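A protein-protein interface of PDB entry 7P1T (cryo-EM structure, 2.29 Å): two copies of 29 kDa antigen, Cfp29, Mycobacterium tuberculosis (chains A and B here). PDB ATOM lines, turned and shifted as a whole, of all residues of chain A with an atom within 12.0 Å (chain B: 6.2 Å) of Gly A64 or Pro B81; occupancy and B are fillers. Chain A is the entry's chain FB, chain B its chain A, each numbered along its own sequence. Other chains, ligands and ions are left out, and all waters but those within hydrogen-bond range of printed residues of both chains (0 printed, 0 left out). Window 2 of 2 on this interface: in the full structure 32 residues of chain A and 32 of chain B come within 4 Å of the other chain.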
ATOM      1  N   VAL A  58      -2.596   2.780 -34.115  1.00  0.00           N
ATOM      2  CA  VAL A  58      -1.436   3.513 -33.587  1.00  0.00           C
ATOM      3  C   VAL A  58      -0.933   2.916 -32.282  1.00  0.00           C
ATOM      4  O   VAL A  58      -1.688   2.249 -31.568  1.00  0.00           O
ATOM      5  CB  VAL A  58      -1.702   5.019 -33.363  1.00  0.00           C
ATOM      6  CG1 VAL A  58      -1.050   5.831 -34.466  1.00  0.00           C
ATOM      7  CG2 VAL A  58      -3.184   5.327 -33.247  1.00  0.00           C
ATOM      8  N   LYS A  59       0.339   3.158 -31.970  1.00  0.00           N
ATOM      9  CA  LYS A  59       0.930   2.613 -30.746  1.00  0.00           C
ATOM     10  C   LYS A  59       0.139   3.012 -29.514  1.00  0.00           C
ATOM     11  O   LYS A  59       0.052   4.197 -29.203  1.00  0.00           O
ATOM     12  CB  LYS A  59       2.396   3.040 -30.599  1.00  0.00           C
ATOM     13  CG  LYS A  59       3.346   2.461 -31.634  1.00  0.00           C
ATOM     14  CD  LYS A  59       4.760   2.964 -31.412  1.00  0.00           C
ATOM     15  CE  LYS A  59       5.720   2.369 -32.429  1.00  0.00           C
ATOM     16  NZ  LYS A  59       7.110   2.870 -32.244  1.00  0.00           N
ATOM     17  N   ALA A  60      -0.422   2.033 -28.810  1.00  0.00           N
ATOM     18  CA  ALA A  60      -1.231   2.282 -27.610  1.00  0.00           C
ATOM     19  C   ALA A  60      -0.659   3.355 -26.684  1.00  0.00           C
ATOM     20  O   ALA A  60       0.496   3.257 -26.260  1.00  0.00           O
ATOM     21  CB  ALA A  60      -1.412   0.980 -26.841  1.00  0.00           C
ATOM     22  N   PRO A  61      -1.475   4.371 -26.347  1.00  0.00           N
ATOM     23  CA  PRO A  61      -1.018   5.436 -25.445  1.00  0.00           C
ATOM     24  C   PRO A  61      -0.595   4.841 -24.122  1.00  0.00           C
ATOM     25  O   PRO A  61       0.532   5.084 -23.685  1.00  0.00           O
ATOM     26  CB  PRO A  61      -2.259   6.313 -25.244  1.00  0.00           C
ATOM     27  CG  PRO A  61      -3.282   5.828 -26.205  1.00  0.00           C
ATOM     28  CD  PRO A  61      -2.920   4.441 -26.619  1.00  0.00           C
ATOM     29  N   THR A  62      -1.481   4.077 -23.491  1.00  0.00           N
ATOM     30  CA  THR A  62      -1.154   3.414 -22.233  1.00  0.00           C
ATOM     31  C   THR A  62      -1.667   1.981 -22.226  1.00  0.00           C
ATOM     32  O   THR A  62      -2.228   1.504 -23.219  1.00  0.00           O
ATOM     33  CB  THR A  62      -1.720   4.157 -20.992  1.00  0.00           C
ATOM     34  OG1 THR A  62      -3.149   4.268 -21.071  1.00  0.00           O
ATOM     35  CG2 THR A  62      -1.117   5.550 -20.889  1.00  0.00           C
ATOM     36  N   ASN A  63      -1.481   1.289 -21.110  1.00  0.00           N
ATOM     37  CA  ASN A  63      -1.946  -0.088 -20.982  1.00  0.00           C
ATOM     38  C   ASN A  63      -3.463  -0.144 -20.987  1.00  0.00           C
ATOM     39  O   ASN A  63      -4.116   0.636 -20.295  1.00  0.00           O
ATOM     40  CB  ASN A  63      -1.403  -0.722 -19.700  1.00  0.00           C
ATOM     41  CG  ASN A  63       0.008  -0.272 -19.378  1.00  0.00           C
ATOM     42  OD1 ASN A  63       0.211   0.692 -18.639  1.00  0.00           O
ATOM     43  ND2 ASN A  63       0.992  -0.968 -19.934  1.00  0.00           N
ATOM     44  N   GLY A  64      -4.026  -1.062 -21.765  1.00  0.00           N
ATOM     45  CA  GLY A  64      -5.472  -1.211 -21.817  1.00  0.00           C
ATOM     46  C   GLY A  64      -6.188  -0.167 -22.650  1.00  0.00           C
ATOM     47  O   GLY A  64      -7.418  -0.118 -22.649  1.00  0.00           O
ATOM     48  N   VAL A  65      -5.437   0.674 -23.355  1.00  0.00           N
ATOM     49  CA  VAL A  65      -6.050   1.666 -24.211  1.00  0.00           C
ATOM     50  C   VAL A  65      -5.825   1.270 -25.642  1.00  0.00           C
ATOM     51  O   VAL A  65      -4.739   0.869 -26.005  1.00  0.00           O
ATOM     52  CB  VAL A  65      -5.507   3.078 -23.931  1.00  0.00           C
ATOM     53  CG1 VAL A  65      -6.371   4.119 -24.625  1.00  0.00           C
ATOM     54  CG2 VAL A  65      -5.455   3.366 -22.439  1.00  0.00           C
ATOM     55  N   ILE A  66      -6.872   1.314 -26.440  1.00  0.00           N
ATOM     56  CA  ILE A  66      -6.764   0.963 -27.831  1.00  0.00           C
ATOM     57  C   ILE A  66      -7.021   2.219 -28.607  1.00  0.00           C
ATOM     58  O   ILE A  66      -8.078   2.819 -28.484  1.00  0.00           O
ATOM     59  CB  ILE A  66      -7.756  -0.147 -28.226  1.00  0.00           C
ATOM     60  CG1 ILE A  66      -7.442  -1.430 -27.461  1.00  0.00           C
ATOM     61  CG2 ILE A  66      -7.712  -0.407 -29.722  1.00  0.00           C
ATOM     62  CD1 ILE A  66      -8.508  -2.486 -27.607  1.00  0.00           C
ATOM     63  N   ALA A  67      -6.050   2.625 -29.401  1.00  0.00           N
ATOM     64  CA  ALA A  67      -6.171   3.873 -30.141  1.00  0.00           C
ATOM     65  C   ALA A  67      -6.170   3.694 -31.626  1.00  0.00           C
ATOM     66  O   ALA A  67      -5.468   2.846 -32.157  1.00  0.00           O
ATOM     67  CB  ALA A  67      -5.042   4.806 -29.736  1.00  0.00           C
ATOM     68  N   HIS A  68      -6.966   4.495 -32.297  1.00  0.00           N
ATOM     69  CA  HIS A  68      -6.981   4.450 -33.733  1.00  0.00           C
ATOM     70  C   HIS A  68      -7.104   5.831 -34.322  1.00  0.00           C
ATOM     71  O   HIS A  68      -7.944   6.612 -33.913  1.00  0.00           O
ATOM     72  CB  HIS A  68      -8.152   3.596 -34.228  1.00  0.00           C
ATOM     73  CG  HIS A  68      -7.895   2.128 -34.214  1.00  0.00           C
ATOM     74  ND1 HIS A  68      -8.305   1.315 -33.182  1.00  0.00           N
ATOM     75  CD2 HIS A  68      -7.288   1.321 -35.113  1.00  0.00           C
ATOM     76  CE1 HIS A  68      -7.947   0.071 -33.438  1.00  0.00           C
ATOM     77  NE2 HIS A  68      -7.331   0.048 -34.605  1.00  0.00           N
ATOM     78  N   ARG B  79     -10.345   3.777 -26.983  1.00  0.00           N
ATOM     79  CA  ARG B  79     -11.249   2.738 -26.517  1.00  0.00           C
ATOM     80  C   ARG B  79     -10.627   2.027 -25.330  1.00  0.00           C
ATOM     81  O   ARG B  79      -9.472   1.593 -25.392  1.00  0.00           O
ATOM     82  CB  ARG B  79     -11.560   1.742 -27.633  1.00  0.00           C
ATOM     83  CG  ARG B  79     -12.359   0.543 -27.185  1.00  0.00           C
ATOM     84  CD  ARG B  79     -12.648  -0.397 -28.327  1.00  0.00           C
ATOM     85  NE  ARG B  79     -13.701   0.109 -29.193  1.00  0.00           N
ATOM     86  CZ  ARG B  79     -14.212  -0.574 -30.208  1.00  0.00           C
ATOM     87  NH1 ARG B  79     -13.759  -1.788 -30.477  1.00  0.00           N
ATOM     88  NH2 ARG B  79     -15.175  -0.049 -30.948  1.00  0.00           N
ATOM     89  N   VAL B  80     -11.388   1.926 -24.251  1.00  0.00           N
ATOM     90  CA  VAL B  80     -10.986   1.214 -23.048  1.00  0.00           C
ATOM     91  C   VAL B  80     -11.977   0.082 -22.816  1.00  0.00           C
ATOM     92  O   VAL B  80     -13.113   0.314 -22.406  1.00  0.00           O
ATOM     93  CB  VAL B  80     -10.928   2.149 -21.827  1.00  0.00           C
ATOM     94  CG1 VAL B  80     -10.404   1.397 -20.617  1.00  0.00           C
ATOM     95  CG2 VAL B  80     -10.073   3.368 -22.117  1.00  0.00           C
ATOM     96  N   PRO B  81     -11.599  -1.152 -23.117  1.00  0.00           N
ATOM     97  CA  PRO B  81     -12.485  -2.282 -22.820  1.00  0.00           C
ATOM     98  C   PRO B  81     -12.518  -2.592 -21.333  1.00  0.00           C
ATOM     99  O   PRO B  81     -11.566  -2.336 -20.597  1.00  0.00           O
ATOM    100  CB  PRO B  81     -11.859  -3.436 -23.610  1.00  0.00           C
ATOM    101  CG  PRO B  81     -10.426  -3.080 -23.700  1.00  0.00           C
ATOM    102  CD  PRO B  81     -10.343  -1.583 -23.756  1.00  0.00           C
ATOM    103  N   PHE B  82     -13.641  -3.153 -20.897  1.00  0.00           N
ATOM    104  CA  PHE B  82     -13.796  -3.606 -19.522  1.00  0.00           C
ATOM    105  C   PHE B  82     -14.784  -4.759 -19.494  1.00  0.00           C
ATOM    106  O   PHE B  82     -15.527  -4.988 -20.447  1.00  0.00           O
ATOM    107  CB  PHE B  82     -14.236  -2.474 -18.578  1.00  0.00           C
ATOM    108  CG  PHE B  82     -15.579  -1.883 -18.895  1.00  0.00           C
ATOM    109  CD1 PHE B  82     -15.726  -0.946 -19.904  1.00  0.00           C
ATOM    110  CD2 PHE B  82     -16.696  -2.244 -18.155  1.00  0.00           C
ATOM    111  CE1 PHE B  82     -16.959  -0.401 -20.189  1.00  0.00           C
ATOM    112  CE2 PHE B  82     -17.933  -1.698 -18.433  1.00  0.00           C
ATOM    113  CZ  PHE B  82     -18.063  -0.773 -19.450  1.00  0.00           C
ATOM    114  N   THR B  83     -14.767  -5.500 -18.393  1.00  0.00           N
ATOM    115  CA  THR B  83     -15.475  -6.766 -18.283  1.00  0.00           C
ATOM    116  C   THR B  83     -16.363  -6.767 -17.049  1.00  0.00           C
ATOM    117  O   THR B  83     -15.886  -6.516 -15.939  1.00  0.00           O
ATOM    118  CB  THR B  83     -14.478  -7.921 -18.220  1.00  0.00           C
ATOM    119  OG1 THR B  83     -13.694  -7.937 -19.416  1.00  0.00           O
ATOM    120  CG2 THR B  83     -15.193  -9.232 -18.094  1.00  0.00           C
ATOM    121  N   ALA B 107     -12.403   1.673 -15.902  1.00  0.00           N
ATOM    122  CA  ALA B 107     -12.393   2.084 -17.300  1.00  0.00           C
ATOM    123  C   ALA B 107     -12.613   3.585 -17.445  1.00  0.00           C
ATOM    124  O   ALA B 107     -11.958   4.233 -18.268  1.00  0.00           O
ATOM    125  CB  ALA B 107     -13.449   1.305 -18.081  1.00  0.00           C
ATOM    126  N   LYS B 110      -9.439   5.318 -16.363  1.00  0.00           N
ATOM    127  CA  LYS B 110      -8.374   5.174 -17.344  1.00  0.00           C
ATOM    128  C   LYS B 110      -8.625   6.036 -18.578  1.00  0.00           C
ATOM    129  O   LYS B 110      -7.694   6.653 -19.106  1.00  0.00           O
ATOM    130  CB  LYS B 110      -8.211   3.704 -17.714  1.00  0.00           C
ATOM    131  CG  LYS B 110      -7.048   3.440 -18.623  1.00  0.00           C
ATOM    132  CD  LYS B 110      -6.966   1.987 -19.001  1.00  0.00           C
ATOM    133  CE  LYS B 110      -6.472   1.167 -17.825  1.00  0.00           C
ATOM    134  NZ  LYS B 110      -6.259  -0.254 -18.180  1.00  0.00           N
ATOM    135  N   LEU B 244     -17.510  -5.003 -22.530  1.00  0.00           N
ATOM    136  CA  LEU B 244     -17.969  -3.749 -23.096  1.00  0.00           C
ATOM    137  C   LEU B 244     -16.764  -2.832 -23.244  1.00  0.00           C
ATOM    138  O   LEU B 244     -15.638  -3.247 -22.977  1.00  0.00           O
ATOM    139  CB  LEU B 244     -19.013  -3.101 -22.189  1.00  0.00           C
ATOM    140  CG  LEU B 244     -20.247  -3.922 -21.815  1.00  0.00           C
ATOM    141  CD1 LEU B 244     -20.628  -3.699 -20.361  1.00  0.00           C
ATOM    142  CD2 LEU B 244     -21.411  -3.594 -22.733  1.00  0.00           C
ATOM    143  N   TYR B 245     -16.982  -1.592 -23.666  1.00  0.00           N
ATOM    144  CA  TYR B 245     -15.898  -0.629 -23.775  1.00  0.00           C
ATOM    145  C   TYR B 245     -16.439   0.776 -23.581  1.00  0.00           C
ATOM    146  O   TYR B 245     -17.621   1.052 -23.801  1.00  0.00           O
ATOM    147  CB  TYR B 245     -15.150  -0.738 -25.121  1.00  0.00           C
ATOM    148  CG  TYR B 245     -16.017  -0.658 -26.359  1.00  0.00           C
ATOM    149  CD1 TYR B 245     -16.405   0.568 -26.891  1.00  0.00           C
ATOM    150  CD2 TYR B 245     -16.456  -1.810 -26.990  1.00  0.00           C
ATOM    151  CE1 TYR B 245     -17.198   0.637 -28.016  1.00  0.00           C
ATOM    152  CE2 TYR B 245     -17.254  -1.749 -28.111  1.00  0.00           C
ATOM    153  CZ  TYR B 245     -17.620  -0.523 -28.617  1.00  0.00           C
ATOM    154  OH  TYR B 245     -18.412  -0.449 -29.732  1.00  0.00           O
ATOM    155  N   LEU B 246     -15.541   1.659 -23.175  1.00  0.00           N
ATOM    156  CA  LEU B 246     -15.761   3.093 -23.193  1.00  0.00           C
ATOM    157  C   LEU B 246     -15.020   3.651 -24.394  1.00  0.00           C
ATOM    158  O   LEU B 246     -13.915   3.204 -24.704  1.00  0.00           O
ATOM    159  CB  LEU B 246     -15.245   3.742 -21.916  1.00  0.00           C
ATOM    160  CG  LEU B 246     -15.873   3.276 -20.608  1.00  0.00           C
ATOM    161  CD1 LEU B 246     -15.553   4.277 -19.564  1.00  0.00           C
ATOM    162  CD2 LEU B 246     -17.359   3.141 -20.718  1.00  0.00           C
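The backbone carbonyl oxygen of Arg B79 lies within hydrogen-bond range of the backbone NH of Ile A66 (2.8 Å).
The side-chain amino group (NZ) of Lys B110 sits at hydrogen-bond distance from the backbone carbonyl oxygen (O) of Asn A63, 3.1 Å away.
The guanidinium group (NH2) of Arg B79 sits close to the side-chain hydroxyl (OH) of Tyr B245 (3.5 Å).
The backbone carbonyl oxygen of Leu B246 sits at hydrogen-bond distance from the backbone NH of Val B80, 2.9 Å away.
O of Gly A64 touches O of Arg B79, at 3.8 Å.
Gly A64 touches Val B80.
Gly A64 touches Pro B81 (O to CD, 3.5 Å).
CA of Gly A64 touches NZ of Lys B110, at 3.8 Å.
Arg B79 touches Val A65.
Gly A64 touches four residues of chain B.
Of the printed residues of chain A, Pro B81 touches Gly A64 (3.5 Å).
Val B80 touches just one residue of chain A: Gly A64.
No residue of chain A comes within 4 Å of Phe B82.
No residue of chain A comes within 4 Å of Thr B83.
Printed residues of chain B within 4 Å of Asn A63: Lys B110 (3.1 Å).
Printed residues of chain B within 4 Å of Val A65: Arg B79 (3.6 Å).
Printed residues of chain B within 4 Å of Ile A66: Arg B79 (2.8 Å).
Of the printed residues of chain A, Arg B79 touches Gly A64, Val A65 and Ile A66.
Printed residues of chain A within 4 Å of Lys B110: Asn A63 (3.1 Å) and Gly A64 (3.8 Å).
The nearest residue of chain A that does not touch Pro B81 is Ile A66 (4.4 Å).
The nearest printed residue of chain B that does not touch Ile A66 is Pro B81 (4.4 Å).
Of the 11 printed residues of chain A, 4 touch a printed residue of chain B.
Hydrophobic or aromatic side chains of chain A within 4 Å of the printed part of chain B: Ile A66.
Along chain A the printed residues that touch a printed residue of chain B span positions 63 to 66.
Of the 10 printed residues of chain B, 4 touch a printed residue of chain A.
Hydrophobic or aromatic side chains of chain B that line the printed part of chain A: Val B80 and Pro B81.
Among the printed residues, no Asp or Glu carboxylate lies within 4 Å of a Lys or Arg side-chain nitrogen of the other chain.
No position is printed for both chains.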
